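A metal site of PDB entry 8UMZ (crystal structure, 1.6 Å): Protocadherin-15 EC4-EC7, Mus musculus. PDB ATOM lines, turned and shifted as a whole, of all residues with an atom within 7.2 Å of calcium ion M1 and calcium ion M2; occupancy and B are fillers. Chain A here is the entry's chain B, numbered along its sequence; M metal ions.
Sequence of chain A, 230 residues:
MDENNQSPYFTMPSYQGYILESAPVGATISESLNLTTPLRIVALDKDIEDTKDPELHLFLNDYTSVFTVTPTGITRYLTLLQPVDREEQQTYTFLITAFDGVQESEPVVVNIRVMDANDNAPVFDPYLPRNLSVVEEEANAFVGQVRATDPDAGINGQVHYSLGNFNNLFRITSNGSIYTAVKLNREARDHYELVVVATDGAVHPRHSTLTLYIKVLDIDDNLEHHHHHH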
ATOM      1  N   GLU A  21     -12.388   3.689   5.218  1.00  0.00           N
ATOM      2  CA  GLU A  21     -11.395   4.180   6.169  1.00  0.00           C
ATOM      3  C   GLU A  21     -10.505   5.289   5.591  1.00  0.00           C
ATOM      4  O   GLU A  21      -9.993   6.130   6.336  1.00  0.00           O
ATOM      5  CB  GLU A  21     -10.497   3.057   6.701  1.00  0.00           C
ATOM      6  CG  GLU A  21      -9.507   2.505   5.644  1.00  0.00           C
ATOM      7  CD  GLU A  21      -8.677   1.425   6.270  1.00  0.00           C
ATOM      8  OE1 GLU A  21      -8.220   1.518   7.469  1.00  0.00           O
ATOM      9  OE2 GLU A  21      -8.327   0.520   5.523  1.00  0.00           O
ATOM     10  N   ASP A  85      -9.596   3.855  10.918  1.00  0.00           N
ATOM     11  CA  ASP A  85      -8.641   2.839  10.501  1.00  0.00           C
ATOM     12  C   ASP A  85      -9.224   1.455  10.768  1.00  0.00           C
ATOM     13  O   ASP A  85      -9.182   1.000  11.913  1.00  0.00           O
ATOM     14  CB  ASP A  85      -7.331   2.983  11.301  1.00  0.00           C
ATOM     15  CG  ASP A  85      -6.283   1.946  10.960  1.00  0.00           C
ATOM     16  OD1 ASP A  85      -6.443   1.311   9.905  1.00  0.00           O
ATOM     17  OD2 ASP A  85      -5.284   1.785  11.719  1.00  0.00           O
ATOM     18  N   ARG A  86      -9.670   0.764   9.704  1.00  0.00           N
ATOM     19  CA  ARG A  86     -10.291  -0.546   9.839  1.00  0.00           C
ATOM     20  C   ARG A  86      -9.309  -1.485  10.543  1.00  0.00           C
ATOM     21  O   ARG A  86      -9.722  -2.365  11.326  1.00  0.00           O
ATOM     22  CB  ARG A  86     -10.761  -1.034   8.457  1.00  0.00           C
ATOM     23  CG  ARG A  86     -11.612  -2.295   8.541  1.00  0.00           C
ATOM     24  CD  ARG A  86     -11.479  -3.241   7.350  1.00  0.00           C
ATOM     25  NE  ARG A  86     -10.129  -3.753   7.163  1.00  0.00           N
ATOM     26  CZ  ARG A  86      -9.622  -4.786   7.826  1.00  0.00           C
ATOM     27  NH1 ARG A  86      -8.388  -5.159   7.609  1.00  0.00           N
ATOM     28  NH2 ARG A  86     -10.370  -5.456   8.697  1.00  0.00           N
ATOM     29  N   GLU A  87      -7.993  -1.305  10.310  1.00  0.00           N
ATOM     30  CA  GLU A  87      -6.995  -2.221  10.850  1.00  0.00           C
ATOM     31  C   GLU A  87      -6.824  -2.071  12.367  1.00  0.00           C
ATOM     32  O   GLU A  87      -6.221  -2.951  13.014  1.00  0.00           O
ATOM     33  CB  GLU A  87      -5.620  -2.069  10.189  1.00  0.00           C
ATOM     34  CG  GLU A  87      -5.453  -2.754   8.846  1.00  0.00           C
ATOM     35  CD  GLU A  87      -6.196  -2.097   7.689  1.00  0.00           C
ATOM     36  OE1 GLU A  87      -6.035  -0.892   7.535  1.00  0.00           O
ATOM     37  OE2 GLU A  87      -6.878  -2.834   6.896  1.00  0.00           O
ATOM     38  N   MET A 115     -15.294   0.508   6.466  1.00  0.00           N
ATOM     39  CA  MET A 115     -14.952  -0.410   5.388  1.00  0.00           C
ATOM     40  C   MET A 115     -13.449  -0.337   5.052  1.00  0.00           C
ATOM     41  O   MET A 115     -12.777   0.687   5.174  1.00  0.00           O
ATOM     42  CB  MET A 115     -15.852  -0.046   4.203  1.00  0.00           C
ATOM     43  CG  MET A 115     -17.302   0.017   4.624  1.00  0.00           C
ATOM     44  SD  MET A 115     -17.870  -1.437   5.635  1.00  0.00           S
ATOM     45  CE  MET A 115     -17.568  -2.794   4.499  1.00  0.00           C
ATOM     46  N   ASP A 116     -12.885  -1.433   4.555  1.00  0.00           N
ATOM     47  CA  ASP A 116     -11.486  -1.477   4.140  1.00  0.00           C
ATOM     48  C   ASP A 116     -11.189  -0.663   2.889  1.00  0.00           C
ATOM     49  O   ASP A 116     -11.948  -0.652   1.942  1.00  0.00           O
ATOM     50  CB  ASP A 116     -11.084  -2.927   3.864  1.00  0.00           C
ATOM     51  CG  ASP A 116      -9.592  -3.070   3.807  1.00  0.00           C
ATOM     52  OD1 ASP A 116      -8.967  -2.464   4.675  1.00  0.00           O
ATOM     53  OD2 ASP A 116      -9.120  -3.878   2.970  1.00  0.00           O
ATOM     54  N   ALA A 117     -10.091   0.059   2.937  1.00  0.00           N
ATOM     55  CA  ALA A 117      -9.408   0.595   1.769  1.00  0.00           C
ATOM     56  C   ALA A 117      -8.126  -0.193   1.695  1.00  0.00           C
ATOM     57  O   ALA A 117      -7.683  -0.605   2.794  1.00  0.00           O
ATOM     58  CB  ALA A 117      -9.072   2.059   1.990  1.00  0.00           C
ATOM     59  N   ASN A 118      -7.591  -0.387   0.482  1.00  0.00           N
ATOM     60  CA  ASN A 118      -6.297  -1.031   0.350  1.00  0.00           C
ATOM     61  C   ASN A 118      -5.256   0.079   0.561  1.00  0.00           C
ATOM     62  O   ASN A 118      -4.796   0.712  -0.392  1.00  0.00           O
ATOM     63  CB  ASN A 118      -6.174  -1.809  -0.973  1.00  0.00           C
ATOM     64  CG  ASN A 118      -4.864  -2.568  -1.180  1.00  0.00           C
ATOM     65  OD1 ASN A 118      -4.364  -3.422  -0.388  1.00  0.00           O
ATOM     66  ND2 ASN A 118      -4.290  -2.298  -2.359  1.00  0.00           N
ATOM     67  N   ASP A 119      -4.914   0.281   1.835  1.00  0.00           N
ATOM     68  CA  ASP A 119      -4.060   1.368   2.306  1.00  0.00           C
ATOM     69  C   ASP A 119      -2.751   0.764   2.835  1.00  0.00           C
ATOM     70  O   ASP A 119      -1.901   1.484   3.351  1.00  0.00           O
ATOM     71  CB  ASP A 119      -4.778   2.301   3.303  1.00  0.00           C
ATOM     72  CG  ASP A 119      -5.481   1.638   4.496  1.00  0.00           C
ATOM     73  OD1 ASP A 119      -5.472   0.364   4.522  1.00  0.00           O
ATOM     74  OD2 ASP A 119      -6.107   2.388   5.407  1.00  0.00           O
ATOM     75  N   ASN A 120      -2.601  -0.561   2.669  1.00  0.00           N
ATOM     76  CA  ASN A 120      -1.370  -1.232   3.042  1.00  0.00           C
ATOM     77  C   ASN A 120      -0.869  -1.947   1.792  1.00  0.00           C
ATOM     78  O   ASN A 120      -1.646  -2.417   0.954  1.00  0.00           O
ATOM     79  CB  ASN A 120      -1.549  -2.111   4.285  1.00  0.00           C
ATOM     80  CG  ASN A 120      -1.926  -1.345   5.532  1.00  0.00           C
ATOM     81  OD1 ASN A 120      -3.095  -1.331   5.926  1.00  0.00           O
ATOM     82  ND2 ASN A 120      -0.926  -0.781   6.203  1.00  0.00           N
ATOM     83  N   ALA A 121       0.457  -1.926   1.650  1.00  0.00           N
ATOM     84  CA  ALA A 121       1.127  -2.799   0.705  1.00  0.00           C
ATOM     85  C   ALA A 121       1.745  -3.930   1.503  1.00  0.00           C
ATOM     86  O   ALA A 121       2.070  -3.764   2.660  1.00  0.00           O
ATOM     87  CB  ALA A 121       2.199  -2.029  -0.050  1.00  0.00           C
ATOM     88  N   PRO A 122       1.955  -5.101   0.876  1.00  0.00           N
ATOM     89  CA  PRO A 122       2.603  -6.216   1.552  1.00  0.00           C
ATOM     90  C   PRO A 122       3.907  -5.728   2.138  1.00  0.00           C
ATOM     91  O   PRO A 122       4.573  -4.863   1.554  1.00  0.00           O
ATOM     92  CB  PRO A 122       2.742  -7.269   0.415  1.00  0.00           C
ATOM     93  CG  PRO A 122       1.589  -6.896  -0.505  1.00  0.00           C
ATOM     94  CD  PRO A 122       1.656  -5.382  -0.538  1.00  0.00           C
ATOM     95  N   ASP A 150       0.006  -8.799   4.397  1.00  0.00           N
ATOM     96  CA  ASP A 150      -0.752  -7.597   4.131  1.00  0.00           C
ATOM     97  C   ASP A 150      -1.952  -7.583   5.058  1.00  0.00           C
ATOM     98  O   ASP A 150      -2.693  -8.559   5.069  1.00  0.00           O
ATOM     99  CB  ASP A 150      -1.119  -7.597   2.661  1.00  0.00           C
ATOM    100  CG  ASP A 150      -1.683  -6.298   2.155  1.00  0.00           C
ATOM    101  OD1 ASP A 150      -2.532  -5.663   2.893  1.00  0.00           O
ATOM    102  OD2 ASP A 150      -1.288  -5.904   1.038  1.00  0.00           O
ATOM    103  N   PRO A 151      -2.150  -6.537   5.882  1.00  0.00           N
ATOM    104  CA  PRO A 151      -3.204  -6.589   6.891  1.00  0.00           C
ATOM    105  C   PRO A 151      -4.518  -6.006   6.365  1.00  0.00           C
ATOM    106  O   PRO A 151      -5.478  -5.928   7.108  1.00  0.00           O
ATOM    107  CB  PRO A 151      -2.586  -5.714   7.967  1.00  0.00           C
ATOM    108  CG  PRO A 151      -1.985  -4.585   7.188  1.00  0.00           C
ATOM    109  CD  PRO A 151      -1.364  -5.294   5.980  1.00  0.00           C
ATOM    110  N   ASP A 152      -4.595  -5.640   5.099  1.00  0.00           N
ATOM    111  CA  ASP A 152      -5.896  -5.257   4.567  1.00  0.00           C
ATOM    112  C   ASP A 152      -6.837  -6.489   4.413  1.00  0.00           C
ATOM    113  O   ASP A 152      -6.462  -7.655   4.596  1.00  0.00           O
ATOM    114  CB  ASP A 152      -5.839  -4.547   3.242  1.00  0.00           C
ATOM    115  CG  ASP A 152      -4.988  -3.304   3.250  1.00  0.00           C
ATOM    116  OD1 ASP A 152      -5.252  -2.449   4.127  1.00  0.00           O
ATOM    117  OD2 ASP A 152      -4.154  -3.160   2.295  1.00  0.00           O
ATOM    118  N   ALA A 153      -8.080  -6.173   4.113  1.00  0.00           N
ATOM    119  CA  ALA A 153      -9.176  -7.137   4.074  1.00  0.00           C
ATOM    120  C   ALA A 153      -9.459  -7.657   2.680  1.00  0.00           C
ATOM    121  O   ALA A 153      -9.408  -6.936   1.676  1.00  0.00           O
ATOM    122  CB  ALA A 153     -10.427  -6.461   4.495  1.00  0.00           C
ATOM    123  N   ILE A 155      -9.708  -9.300  -0.924  1.00  0.00           N
ATOM    124  CA  ILE A 155      -8.686  -9.291  -1.969  1.00  0.00           C
ATOM    125  C   ILE A 155      -7.568  -8.305  -1.650  1.00  0.00           C
ATOM    126  O   ILE A 155      -6.418  -8.562  -1.974  1.00  0.00           O
ATOM    127  CB  ILE A 155      -9.259  -8.997  -3.379  1.00  0.00           C
ATOM    128  CG1 ILE A 155     -10.043  -7.683  -3.418  1.00  0.00           C
ATOM    129  CG2 ILE A 155     -10.026 -10.193  -3.916  1.00  0.00           C
ATOM    130  CD1 ILE A 155     -10.898  -7.538  -4.666  1.00  0.00           C
ATOM    131  N   ASN A 156      -7.876  -7.176  -0.959  1.00  0.00           N
ATOM    132  CA  ASN A 156      -6.857  -6.173  -0.675  1.00  0.00           C
ATOM    133  C   ASN A 156      -5.738  -6.680   0.220  1.00  0.00           C
ATOM    134  O   ASN A 156      -4.665  -6.089   0.204  1.00  0.00           O
ATOM    135  CB  ASN A 156      -7.434  -4.941   0.007  1.00  0.00           C
ATOM    136  CG  ASN A 156      -8.540  -4.348  -0.828  1.00  0.00           C
ATOM    137  OD1 ASN A 156      -8.562  -4.466  -2.054  1.00  0.00           O
ATOM    138  ND2 ASN A 156      -9.462  -3.657  -0.179  1.00  0.00           N
ATOM    139  N   GLY A 157      -6.009  -7.678   1.072  1.00  0.00           N
ATOM    140  CA  GLY A 157      -4.990  -8.261   1.924  1.00  0.00           C
ATOM    141  C   GLY A 157      -4.403  -9.567   1.383  1.00  0.00           C
ATOM    142  O   GLY A 157      -3.570 -10.178   2.052  1.00  0.00           O
ATOM    143  N   GLN A 158      -4.813 -10.023   0.179  1.00  0.00           N
ATOM    144  CA  GLN A 158      -4.349 -11.311  -0.327  1.00  0.00           C
ATOM    145  C   GLN A 158      -3.122 -11.108  -1.239  1.00  0.00           C
ATOM    146  O   GLN A 158      -3.250 -10.360  -2.221  1.00  0.00           O
ATOM    147  CB  GLN A 158      -5.481 -11.997  -1.096  1.00  0.00           C
ATOM    148  CG  GLN A 158      -6.500 -12.723  -0.245  1.00  0.00           C
ATOM    149  CD  GLN A 158      -5.809 -13.783   0.566  1.00  0.00           C
ATOM    150  OE1 GLN A 158      -5.017 -14.572   0.057  1.00  0.00           O
ATOM    151  NE2 GLN A 158      -6.003 -13.734   1.866  1.00  0.00           N
ATOM    152  N   VAL A 159      -2.022 -11.816  -0.925  1.00  0.00           N
ATOM    153  CA  VAL A 159      -0.657 -11.569  -1.386  1.00  0.00           C
ATOM    154  C   VAL A 159      -0.276 -12.639  -2.445  1.00  0.00           C
ATOM    155  O   VAL A 159      -0.326 -13.835  -2.158  1.00  0.00           O
ATOM    156  CB  VAL A 159       0.345 -11.556  -0.215  1.00  0.00           C
ATOM    157  CG1 VAL A 159       1.817 -11.639  -0.633  1.00  0.00           C
ATOM    158  CG2 VAL A 159       0.099 -10.352   0.700  1.00  0.00           C
ATOM    159  N   THR A 199       2.523  -8.569  -4.409  1.00  0.00           N
ATOM    160  CA  THR A 199       1.423  -7.802  -4.943  1.00  0.00           C
ATOM    161  C   THR A 199       0.133  -8.270  -4.281  1.00  0.00           C
ATOM    162  O   THR A 199      -0.085  -9.466  -4.140  1.00  0.00           O
ATOM    163  CB  THR A 199       1.323  -7.963  -6.467  1.00  0.00           C
ATOM    164  OG1 THR A 199       2.587  -7.652  -7.060  1.00  0.00           O
ATOM    165  CG2 THR A 199       0.256  -7.056  -7.048  1.00  0.00           C
ATOM    166  N   ASP A 200      -0.739  -7.316  -3.895  1.00  0.00           N
ATOM    167  CA  ASP A 200      -2.039  -7.699  -3.406  1.00  0.00           C
ATOM    168  C   ASP A 200      -3.050  -7.794  -4.547  1.00  0.00           C
ATOM    169  O   ASP A 200      -2.682  -7.715  -5.717  1.00  0.00           O
ATOM    170  CB  ASP A 200      -2.390  -6.776  -2.227  1.00  0.00           C
ATOM    171  CG  ASP A 200      -2.568  -5.337  -2.620  1.00  0.00           C
ATOM    172  OD1 ASP A 200      -2.991  -5.105  -3.747  1.00  0.00           O
ATOM    173  OD2 ASP A 200      -2.458  -4.446  -1.719  1.00  0.00           O
ATOM    174  N   GLY A 201      -4.298  -8.171  -4.218  1.00  0.00           N
ATOM    175  CA  GLY A 201      -5.319  -8.572  -5.171  1.00  0.00           C
ATOM    176  C   GLY A 201      -6.339  -7.476  -5.461  1.00  0.00           C
ATOM    177  O   GLY A 201      -7.404  -7.741  -5.988  1.00  0.00           O
ATOM    178  N   ALA A 202      -6.018  -6.260  -5.038  1.00  0.00           N
ATOM    179  CA  ALA A 202      -6.964  -5.163  -5.074  1.00  0.00           C
ATOM    180  C   ALA A 202      -7.319  -4.933  -6.532  1.00  0.00           C
ATOM    181  O   ALA A 202      -6.581  -5.365  -7.419  1.00  0.00           O
ATOM    182  CB  ALA A 202      -6.363  -3.956  -4.412  1.00  0.00           C
ATOM    183  N   PRO A 205      -4.045  -2.732  -7.530  1.00  0.00           N
ATOM    184  CA  PRO A 205      -3.119  -3.504  -6.708  1.00  0.00           C
ATOM    185  C   PRO A 205      -1.965  -2.652  -6.220  1.00  0.00           C
ATOM    186  O   PRO A 205      -1.495  -1.794  -6.980  1.00  0.00           O
ATOM    187  CB  PRO A 205      -2.622  -4.647  -7.614  1.00  0.00           C
ATOM    188  CG  PRO A 205      -3.091  -4.311  -9.027  1.00  0.00           C
ATOM    189  CD  PRO A 205      -4.212  -3.299  -8.896  1.00  0.00           C
ATOM    190  N   ARG A 206      -1.506  -2.905  -4.999  1.00  0.00           N
ATOM    191  CA  ARG A 206      -0.285  -2.325  -4.487  1.00  0.00           C
ATOM    192  C   ARG A 206       0.760  -3.431  -4.356  1.00  0.00           C
ATOM    193  O   ARG A 206       0.435  -4.625  -4.187  1.00  0.00           O
ATOM    194  CB  ARG A 206      -0.511  -1.615  -3.138  1.00  0.00           C
ATOM    195  CG  ARG A 206      -1.456  -0.417  -3.217  1.00  0.00           C
ATOM    196  CD  ARG A 206      -1.737   0.271  -1.898  1.00  0.00           C
ATOM    197  NE  ARG A 206      -0.509   0.612  -1.194  1.00  0.00           N
ATOM    198  CZ  ARG A 206      -0.370   1.582  -0.302  1.00  0.00           C
ATOM    199  NH1 ARG A 206      -1.380   2.392  -0.023  1.00  0.00           N
ATOM    200  NH2 ARG A 206       0.799   1.763   0.298  1.00  0.00           N
HETATM  201 CA    CA M   1      -3.109  -4.276   0.633  1.00  0.00          CA
HETATM  202 CA    CA M   2      -7.053  -1.323   5.125  1.00  0.00          CA
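Within 4 Å of calcium ion M1: Asn 118, Asn 120, Asp 150, Asp 152, Asn 156 and Asp 200.
Calcium ion M2 is bound by the side-chain carboxylate (OD1) of Asp 116 (2.3 Å), the side-chain carboxylate (OE2) of Glu 21 (2.3 Å), the side-chain carboxylate (OE2) of Glu 87 (2.3 Å), the side-chain carboxylate (OD1) of Asp 152 (2.3 Å), the side-chain carboxylate (OD1) of Asp 119 (2.4 Å), the backbone carbonyl oxygen (O) of Ala 117 (2.5 Å) and the side-chain carboxylate (OE1) of Glu 87 (2.7 Å).
Calcium ion M2 has seven donor atoms within binding distance.
OD2 of Asp 116 lies within hydrogen-bond range of ND2 of Asn 156.
NE of Arg 86 lies close to OD1 of Asp 116, at 3.0 Å.
OE1 of Glu 21 lies within hydrogen-bond range of N of Arg 86, 2.8 Å away.
The side-chain carboxylate (OE1) of Glu 87 lies close to the side-chain amide oxygen (OD1) of Asn 120 (3.4 Å).
NH1 of Arg 86 lies close to OE2 of Glu 87 (2.9 Å).
The backbone NH (N) of Glu 87 lies close to the side-chain carboxylate (OD1) of Asp 85.
OD1 of Asp 200 is in hydrogen-bond range of N of Arg 206 (2.9 Å).
The side-chain carboxylate (OD1) of Asp 200 lies close to the backbone NH (N) of Ala 202.
Of the 27 residues printed, 6 come within 4 Å of calcium ion M2.
Calcium ion M1 is bound by OD1 of Asn 118 (1.8 Å), OD2 of Asp 152 (2.3 Å), O of Asn 120 (2.4 Å), O of Asn 156 (2.4 Å), OD2 of Asp 200 (2.4 Å), OD2 of Asp 150 (2.5 Å) and OD1 of Asp 150 (2.7 Å).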
